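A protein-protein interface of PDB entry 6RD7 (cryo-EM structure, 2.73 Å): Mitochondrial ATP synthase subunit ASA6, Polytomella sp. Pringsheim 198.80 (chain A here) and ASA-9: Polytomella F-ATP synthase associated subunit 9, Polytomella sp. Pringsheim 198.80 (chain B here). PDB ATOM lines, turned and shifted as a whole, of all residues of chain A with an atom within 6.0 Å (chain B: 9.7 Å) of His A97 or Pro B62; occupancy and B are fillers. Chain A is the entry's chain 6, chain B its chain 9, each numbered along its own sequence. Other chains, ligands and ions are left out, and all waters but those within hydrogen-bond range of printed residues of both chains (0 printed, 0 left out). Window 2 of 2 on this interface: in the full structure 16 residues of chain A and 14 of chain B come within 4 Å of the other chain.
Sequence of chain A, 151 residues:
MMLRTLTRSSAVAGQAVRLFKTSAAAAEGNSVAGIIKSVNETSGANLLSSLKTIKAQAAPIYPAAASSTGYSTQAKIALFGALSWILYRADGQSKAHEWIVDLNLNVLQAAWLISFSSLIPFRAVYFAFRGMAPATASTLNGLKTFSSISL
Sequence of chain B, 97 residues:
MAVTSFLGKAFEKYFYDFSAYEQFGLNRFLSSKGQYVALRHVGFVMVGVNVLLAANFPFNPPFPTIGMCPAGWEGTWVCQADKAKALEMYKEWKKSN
Pro B62 touches His A97. Pro B62 touches Glu A98. Trp A99 touches Asn B56. CZ2 of Trp A99 touches CD2 of Phe B59, at 3.4 Å. Pro B62 touches Trp A99. Pro B62 touches Ile A100 (CD to CG2, 3.7 Å). Phe B63 touches Ile A100.
His A97 touches just one residue of chain B: Pro B62 (3.3 Å). Of the printed residues of chain A, Pro B62 touches His A97 (3.3 Å), Glu A98 (3.8 Å), Trp A99 (3.4 Å) and Ile A100 (3.7 Å). No residue of chain B comes within 4 Å of Ala A96. Of the printed residues of chain B, Trp A99 touches Asn B56, Phe B59 and Pro B62. Printed residues of chain A within 4 Å of Phe B59: Trp A99. Of the printed residues of chain A, Asn B56 touches Trp A99. Ala B81 touches none of the printed residues of chain A. Gln A93 touches none of the printed residues of chain B. The nearest residue of chain B that does not touch His A97 is Lys B83 (6.0 Å). The nearest printed residue of chain B that does not touch Trp A99 is Asn B60 (5.1 Å).
Printed residues of chain B that touch a printed residue of chain A: Asn B56, Phe B59, Pro B62 and Phe B63. Hydrophobic or aromatic side chains of chain B that line the printed part of chain A: Phe B59, Pro B62 and Phe B63. Along chain B the printed residues that touch a printed residue of chain A span positions 56 to 63. Printed residues of chain A that touch a printed residue of chain B: His A97, Glu A98, Trp A99 and Ile A100. Hydrophobic or aromatic side chains of chain A that line the printed part of chain B: Trp A99 and Ile A100. Along chain A the printed residues that touch a printed residue of chain B span positions 97 to 100. Among the printed residues, no Asp or Glu carboxylate lies within 4 Å of a Lys or Arg side-chain nitrogen of the other chain.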
ATOM      1  N   GLN A  93      26.034 -32.242   7.944  1.00  0.00           N
ATOM      2  CA  GLN A  93      24.973 -31.262   7.736  1.00  0.00           C
ATOM      3  C   GLN A  93      24.154 -31.068   8.998  1.00  0.00           C
ATOM      4  O   GLN A  93      23.664 -29.968   9.268  1.00  0.00           O
ATOM      5  CB  GLN A  93      24.062 -31.706   6.595  1.00  0.00           C
ATOM      6  CG  GLN A  93      24.521 -31.296   5.219  1.00  0.00           C
ATOM      7  CD  GLN A  93      23.569 -31.761   4.147  1.00  0.00           C
ATOM      8  OE1 GLN A  93      22.693 -32.585   4.397  1.00  0.00           O
ATOM      9  NE2 GLN A  93      23.736 -31.240   2.942  1.00  0.00           N
ATOM     10  N   SER A  94      23.976 -32.135   9.775  1.00  0.00           N
ATOM     11  CA  SER A  94      23.203 -32.028  11.005  1.00  0.00           C
ATOM     12  C   SER A  94      23.983 -31.277  12.080  1.00  0.00           C
ATOM     13  O   SER A  94      23.401 -30.550  12.888  1.00  0.00           O
ATOM     14  CB  SER A  94      22.801 -33.421  11.476  1.00  0.00           C
ATOM     15  OG  SER A  94      23.935 -34.166  11.875  1.00  0.00           O
ATOM     16  N   LYS A  95      25.306 -31.405  12.089  1.00  0.00           N
ATOM     17  CA  LYS A  95      26.086 -30.675  13.081  1.00  0.00           C
ATOM     18  C   LYS A  95      26.285 -29.208  12.725  1.00  0.00           C
ATOM     19  O   LYS A  95      26.863 -28.469  13.528  1.00  0.00           O
ATOM     20  CB  LYS A  95      27.440 -31.349  13.277  1.00  0.00           C
ATOM     21  CG  LYS A  95      27.352 -32.704  13.938  1.00  0.00           C
ATOM     22  CD  LYS A  95      28.707 -33.369  14.001  1.00  0.00           C
ATOM     23  CE  LYS A  95      28.664 -34.593  14.888  1.00  0.00           C
ATOM     24  NZ  LYS A  95      27.555 -35.495  14.497  1.00  0.00           N
ATOM     25  N   ALA A  96      25.823 -28.763  11.559  1.00  0.00           N
ATOM     26  CA  ALA A  96      26.005 -27.382  11.145  1.00  0.00           C
ATOM     27  C   ALA A  96      25.062 -26.460  11.913  1.00  0.00           C
ATOM     28  O   ALA A  96      24.171 -26.903  12.641  1.00  0.00           O
ATOM     29  CB  ALA A  96      25.774 -27.239   9.643  1.00  0.00           C
ATOM     30  N   HIS A  97      25.266 -25.152  11.732  1.00  0.00           N
ATOM     31  CA  HIS A  97      24.515 -24.167  12.504  1.00  0.00           C
ATOM     32  C   HIS A  97      23.059 -24.102  12.060  1.00  0.00           C
ATOM     33  O   HIS A  97      22.148 -24.294  12.872  1.00  0.00           O
ATOM     34  CB  HIS A  97      25.167 -22.793  12.393  1.00  0.00           C
ATOM     35  CG  HIS A  97      24.269 -21.674  12.819  1.00  0.00           C
ATOM     36  ND1 HIS A  97      23.888 -21.488  14.129  1.00  0.00           N
ATOM     37  CD2 HIS A  97      23.667 -20.692  12.109  1.00  0.00           C
ATOM     38  CE1 HIS A  97      23.091 -20.438  14.210  1.00  0.00           C
ATOM     39  NE2 HIS A  97      22.941 -19.937  12.997  1.00  0.00           N
ATOM     40  N   GLU A  98      22.814 -23.812  10.787  1.00  0.00           N
ATOM     41  CA  GLU A  98      21.464 -23.928  10.238  1.00  0.00           C
ATOM     42  C   GLU A  98      21.277 -25.303   9.601  1.00  0.00           C
ATOM     43  O   GLU A  98      21.211 -25.485   8.392  1.00  0.00           O
ATOM     44  CB  GLU A  98      21.167 -22.786   9.269  1.00  0.00           C
ATOM     45  CG  GLU A  98      22.244 -22.446   8.257  1.00  0.00           C
ATOM     46  CD  GLU A  98      22.001 -21.096   7.611  1.00  0.00           C
ATOM     47  OE1 GLU A  98      21.828 -20.106   8.352  1.00  0.00           O
ATOM     48  OE2 GLU A  98      21.962 -21.026   6.366  1.00  0.00           O
ATOM     49  N   TRP A  99      21.187 -26.279  10.499  1.00  0.00           N
ATOM     50  CA  TRP A  99      21.197 -27.688  10.126  1.00  0.00           C
ATOM     51  C   TRP A  99      19.890 -28.107   9.474  1.00  0.00           C
ATOM     52  O   TRP A  99      19.889 -28.885   8.514  1.00  0.00           O
ATOM     53  CB  TRP A  99      21.458 -28.528  11.372  1.00  0.00           C
ATOM     54  CG  TRP A  99      20.655 -28.096  12.569  1.00  0.00           C
ATOM     55  CD1 TRP A  99      20.974 -27.119  13.466  1.00  0.00           C
ATOM     56  CD2 TRP A  99      19.402 -28.632  12.995  1.00  0.00           C
ATOM     57  NE1 TRP A  99      19.989 -27.000  14.407  1.00  0.00           N
ATOM     58  CE2 TRP A  99      19.015 -27.924  14.144  1.00  0.00           C
ATOM     59  CE3 TRP A  99      18.569 -29.645  12.517  1.00  0.00           C
ATOM     60  CZ2 TRP A  99      17.835 -28.194  14.819  1.00  0.00           C
ATOM     61  CZ3 TRP A  99      17.399 -29.904  13.184  1.00  0.00           C
ATOM     62  CH2 TRP A  99      17.040 -29.181  14.320  1.00  0.00           C
ATOM     63  N   ILE A 100      18.766 -27.611   9.995  1.00  0.00           N
ATOM     64  CA  ILE A 100      17.463 -27.965   9.455  1.00  0.00           C
ATOM     65  C   ILE A 100      17.282 -27.354   8.074  1.00  0.00           C
ATOM     66  O   ILE A 100      16.651 -27.964   7.203  1.00  0.00           O
ATOM     67  CB  ILE A 100      16.377 -27.556  10.476  1.00  0.00           C
ATOM     68  CG1 ILE A 100      14.980 -27.972  10.020  1.00  0.00           C
ATOM     69  CG2 ILE A 100      16.441 -26.077  10.813  1.00  0.00           C
ATOM     70  CD1 ILE A 100      14.663 -29.421  10.275  1.00  0.00           C
ATOM     71  N   VAL A 101      17.906 -26.203   7.834  1.00  0.00           N
ATOM     72  CA  VAL A 101      17.950 -25.581   6.519  1.00  0.00           C
ATOM     73  C   VAL A 101      18.647 -26.487   5.508  1.00  0.00           C
ATOM     74  O   VAL A 101      18.131 -26.711   4.410  1.00  0.00           O
ATOM     75  CB  VAL A 101      18.631 -24.209   6.653  1.00  0.00           C
ATOM     76  CG1 VAL A 101      19.078 -23.672   5.320  1.00  0.00           C
ATOM     77  CG2 VAL A 101      17.688 -23.240   7.339  1.00  0.00           C
ATOM     78  N   LEU B  53      10.207 -31.003  10.169  1.00  0.00           N
ATOM     79  CA  LEU B  53       9.865 -30.179  11.325  1.00  0.00           C
ATOM     80  C   LEU B  53       9.152 -30.992  12.398  1.00  0.00           C
ATOM     81  O   LEU B  53       9.200 -30.644  13.581  1.00  0.00           O
ATOM     82  CB  LEU B  53       9.003 -28.997  10.896  1.00  0.00           C
ATOM     83  CG  LEU B  53       9.743 -27.806  10.303  1.00  0.00           C
ATOM     84  CD1 LEU B  53       8.763 -26.706   9.965  1.00  0.00           C
ATOM     85  CD2 LEU B  53      10.796 -27.305  11.269  1.00  0.00           C
ATOM     86  N   ASN B  56      11.465 -33.277  14.912  1.00  0.00           N
ATOM     87  CA  ASN B  56      11.989 -32.495  16.062  1.00  0.00           C
ATOM     88  C   ASN B  56      11.263 -31.150  16.010  1.00  0.00           C
ATOM     89  O   ASN B  56      11.601 -30.355  15.121  1.00  0.00           O
ATOM     90  CB  ASN B  56      13.507 -32.323  15.986  1.00  0.00           C
ATOM     91  CG  ASN B  56      14.008 -32.114  14.573  1.00  0.00           C
ATOM     92  OD1 ASN B  56      13.250 -31.707  13.697  1.00  0.00           O
ATOM     93  ND2 ASN B  56      15.278 -32.392  14.340  1.00  0.00           N
ATOM     94  N   PHE B  57      10.283 -30.924  16.890  1.00  0.00           N
ATOM     95  CA  PHE B  57       9.500 -29.664  16.815  1.00  0.00           C
ATOM     96  C   PHE B  57       9.737 -28.762  18.029  1.00  0.00           C
ATOM     97  O   PHE B  57       9.483 -27.547  17.913  1.00  0.00           O
ATOM     98  CB  PHE B  57       8.000 -29.947  16.738  1.00  0.00           C
ATOM     99  CG  PHE B  57       7.182 -28.877  17.410  1.00  0.00           C
ATOM    100  CD1 PHE B  57       6.634 -29.081  18.665  1.00  0.00           C
ATOM    101  CD2 PHE B  57       7.016 -27.641  16.812  1.00  0.00           C
ATOM    102  CE1 PHE B  57       5.901 -28.084  19.289  1.00  0.00           C
ATOM    103  CE2 PHE B  57       6.280 -26.646  17.435  1.00  0.00           C
ATOM    104  CZ  PHE B  57       5.726 -26.868  18.672  1.00  0.00           C
ATOM    105  N   PRO B  58      10.178 -29.285  19.193  1.00  0.00           N
ATOM    106  CA  PRO B  58      10.386 -28.448  20.380  1.00  0.00           C
ATOM    107  C   PRO B  58      11.667 -27.602  20.346  1.00  0.00           C
ATOM    108  O   PRO B  58      11.799 -26.742  21.185  1.00  0.00           O
ATOM    109  CB  PRO B  58      10.476 -29.485  21.507  1.00  0.00           C
ATOM    110  CG  PRO B  58      11.070 -30.698  20.832  1.00  0.00           C
ATOM    111  CD  PRO B  58      10.480 -30.696  19.436  1.00  0.00           C
ATOM    112  N   PHE B  59      12.539 -27.834  19.360  1.00  0.00           N
ATOM    113  CA  PHE B  59      13.842 -27.130  19.229  1.00  0.00           C
ATOM    114  C   PHE B  59      13.674 -25.638  18.915  1.00  0.00           C
ATOM    115  O   PHE B  59      12.619 -25.219  18.409  1.00  0.00           O
ATOM    116  CB  PHE B  59      14.645 -27.742  18.080  1.00  0.00           C
ATOM    117  CG  PHE B  59      14.180 -27.322  16.708  1.00  0.00           C
ATOM    118  CD1 PHE B  59      12.913 -27.650  16.258  1.00  0.00           C
ATOM    119  CD2 PHE B  59      14.999 -26.582  15.872  1.00  0.00           C
ATOM    120  CE1 PHE B  59      12.480 -27.262  15.001  1.00  0.00           C
ATOM    121  CE2 PHE B  59      14.562 -26.188  14.617  1.00  0.00           C
ATOM    122  CZ  PHE B  59      13.305 -26.530  14.183  1.00  0.00           C
ATOM    123  N   ASN B  60      14.720 -24.868  19.229  1.00  0.00           N
ATOM    124  CA  ASN B  60      14.810 -23.451  18.912  1.00  0.00           C
ATOM    125  C   ASN B  60      15.310 -23.302  17.481  1.00  0.00           C
ATOM    126  O   ASN B  60      16.315 -23.923  17.117  1.00  0.00           O
ATOM    127  CB  ASN B  60      15.753 -22.759  19.893  1.00  0.00           C
ATOM    128  CG  ASN B  60      15.660 -21.257  19.838  1.00  0.00           C
ATOM    129  OD1 ASN B  60      14.578 -20.689  19.756  1.00  0.00           O
ATOM    130  ND2 ASN B  60      16.804 -20.598  19.905  1.00  0.00           N
ATOM    131  N   PRO B  61      14.645 -22.511  16.646  1.00  0.00           N
ATOM    132  CA  PRO B  61      14.969 -22.486  15.218  1.00  0.00           C
ATOM    133  C   PRO B  61      16.279 -21.771  14.942  1.00  0.00           C
ATOM    134  O   PRO B  61      16.518 -20.666  15.449  1.00  0.00           O
ATOM    135  CB  PRO B  61      13.788 -21.723  14.609  1.00  0.00           C
ATOM    136  CG  PRO B  61      13.242 -20.921  15.719  1.00  0.00           C
ATOM    137  CD  PRO B  61      13.410 -21.766  16.932  1.00  0.00           C
ATOM    138  N   PRO B  62      17.160 -22.378  14.142  1.00  0.00           N
ATOM    139  CA  PRO B  62      18.321 -21.624  13.649  1.00  0.00           C
ATOM    140  C   PRO B  62      17.932 -20.588  12.620  1.00  0.00           C
ATOM    141  O   PRO B  62      18.564 -19.528  12.536  1.00  0.00           O
ATOM    142  CB  PRO B  62      19.222 -22.711  13.046  1.00  0.00           C
ATOM    143  CG  PRO B  62      18.602 -24.020  13.427  1.00  0.00           C
ATOM    144  CD  PRO B  62      17.162 -23.766  13.662  1.00  0.00           C
ATOM    145  N   PHE B  63      16.910 -20.874  11.825  1.00  0.00           N
ATOM    146  CA  PHE B  63      16.418 -19.917  10.852  1.00  0.00           C
ATOM    147  C   PHE B  63      15.691 -18.782  11.566  1.00  0.00           C
ATOM    148  O   PHE B  63      15.060 -19.007  12.602  1.00  0.00           O
ATOM    149  CB  PHE B  63      15.484 -20.598   9.846  1.00  0.00           C
ATOM    150  CG  PHE B  63      14.436 -21.489  10.469  1.00  0.00           C
ATOM    151  CD1 PHE B  63      14.667 -22.847  10.636  1.00  0.00           C
ATOM    152  CD2 PHE B  63      13.203 -20.981  10.840  1.00  0.00           C
ATOM    153  CE1 PHE B  63      13.707 -23.663  11.196  1.00  0.00           C
ATOM    154  CE2 PHE B  63      12.242 -21.796  11.396  1.00  0.00           C
ATOM    155  CZ  PHE B  63      12.491 -23.136  11.570  1.00  0.00           C
ATOM    156  N   PRO B  64      15.780 -17.553  11.057  1.00  0.00           N
ATOM    157  CA  PRO B  64      15.083 -16.436  11.707  1.00  0.00           C
ATOM    158  C   PRO B  64      13.578 -16.548  11.517  1.00  0.00           C
ATOM    159  O   PRO B  64      13.087 -16.708  10.398  1.00  0.00           O
ATOM    160  CB  PRO B  64      15.653 -15.200  11.002  1.00  0.00           C
ATOM    161  CG  PRO B  64      16.153 -15.704   9.699  1.00  0.00           C
ATOM    162  CD  PRO B  64      16.640 -17.095   9.952  1.00  0.00           C
ATOM    163  N   THR B  65      12.852 -16.477  12.626  1.00  0.00           N
ATOM    164  CA  THR B  65      11.404 -16.579  12.599  1.00  0.00           C
ATOM    165  C   THR B  65      10.793 -15.220  12.284  1.00  0.00           C
ATOM    166  O   THR B  65      11.409 -14.175  12.515  1.00  0.00           O
ATOM    167  CB  THR B  65      10.871 -17.117  13.929  1.00  0.00           C
ATOM    168  OG1 THR B  65       9.457 -17.307  13.831  1.00  0.00           O
ATOM    169  CG2 THR B  65      11.183 -16.167  15.079  1.00  0.00           C
ATOM    170  N   TRP B  77      12.205 -21.240  25.752  1.00  0.00           N
ATOM    171  CA  TRP B  77      13.480 -21.347  24.989  1.00  0.00           C
ATOM    172  C   TRP B  77      13.204 -21.350  23.480  1.00  0.00           C
ATOM    173  O   TRP B  77      14.010 -20.767  22.738  1.00  0.00           O
ATOM    174  CB  TRP B  77      14.276 -22.584  25.420  1.00  0.00           C
ATOM    175  CG  TRP B  77      13.469 -23.844  25.463  1.00  0.00           C
ATOM    176  CD1 TRP B  77      12.349 -24.078  26.205  1.00  0.00           C
ATOM    177  CD2 TRP B  77      13.725 -25.056  24.732  1.00  0.00           C
ATOM    178  NE1 TRP B  77      11.891 -25.348  25.987  1.00  0.00           N
ATOM    179  CE2 TRP B  77      12.713 -25.973  25.088  1.00  0.00           C
ATOM    180  CE3 TRP B  77      14.701 -25.454  23.813  1.00  0.00           C
ATOM    181  CZ2 TRP B  77      12.657 -27.259  24.558  1.00  0.00           C
ATOM    182  CZ3 TRP B  77      14.644 -26.726  23.291  1.00  0.00           C
ATOM    183  CH2 TRP B  77      13.640 -27.618  23.666  1.00  0.00           C
ATOM    184  N   VAL B  78      12.097 -21.974  23.060  1.00  0.00           N
ATOM    185  CA  VAL B  78      11.654 -22.078  21.637  1.00  0.00           C
ATOM    186  C   VAL B  78      11.412 -20.679  21.049  1.00  0.00           C
ATOM    187  O   VAL B  78      11.556 -20.538  19.824  1.00  0.00           O
ATOM    188  CB  VAL B  78      10.395 -22.955  21.515  1.00  0.00           C
ATOM    189  CG1 VAL B  78      10.175 -23.435  20.091  1.00  0.00           C
ATOM    190  CG2 VAL B  78      10.439 -24.129  22.478  1.00  0.00           C
ATOM    191  N   GLN B  80      13.019 -17.709  21.907  1.00  0.00           N
ATOM    192  CA  GLN B  80      14.050 -16.825  22.428  1.00  0.00           C
ATOM    193  C   GLN B  80      14.970 -16.422  21.286  1.00  0.00           C
ATOM    194  O   GLN B  80      15.593 -17.283  20.656  1.00  0.00           O
ATOM    195  CB  GLN B  80      14.838 -17.502  23.547  1.00  0.00           C
ATOM    196  CG  GLN B  80      15.197 -16.574  24.690  1.00  0.00           C
ATOM    197  CD  GLN B  80      14.007 -15.786  25.187  1.00  0.00           C
ATOM    198  OE1 GLN B  80      12.994 -16.356  25.588  1.00  0.00           O
ATOM    199  NE2 GLN B  80      14.121 -14.465  25.160  1.00  0.00           N
ATOM    200  N   ALA B  81      15.044 -15.117  21.018  1.00  0.00           N
ATOM    201  CA  ALA B  81      15.947 -14.631  19.981  1.00  0.00           C
ATOM    202  C   ALA B  81      17.399 -14.741  20.423  1.00  0.00           C
ATOM    203  O   ALA B  81      18.294 -14.937  19.595  1.00  0.00           O
ATOM    204  CB  ALA B  81      15.607 -13.187  19.618  1.00  0.00           C
ATOM    205  N   LYS B  83      20.315 -16.767  21.828  1.00  0.00           N
ATOM    206  CA  LYS B  83      20.537 -18.208  21.760  1.00  0.00           C
ATOM    207  C   LYS B  83      21.210 -18.733  23.020  1.00  0.00           C
ATOM    208  O   LYS B  83      20.992 -19.885  23.407  1.00  0.00           O
ATOM    209  CB  LYS B  83      21.362 -18.551  20.523  1.00  0.00           C
ATOM    210  CG  LYS B  83      20.758 -18.050  19.228  1.00  0.00           C
ATOM    211  CD  LYS B  83      19.394 -18.670  18.989  1.00  0.00           C
ATOM    212  CE  LYS B  83      18.645 -17.963  17.877  1.00  0.00           C
ATOM    213  NZ  LYS B  83      17.315 -18.576  17.629  1.00  0.00           N
ATOM    214  N   ALA B  86      18.453 -19.024  25.293  1.00  0.00           N
ATOM    215  CA  ALA B  86      17.647 -20.181  24.920  1.00  0.00           C
ATOM    216  C   ALA B  86      18.293 -21.484  25.376  1.00  0.00           C
ATOM    217  O   ALA B  86      17.594 -22.415  25.782  1.00  0.00           O
ATOM    218  CB  ALA B  86      17.411 -20.199  23.410  1.00  0.00           C
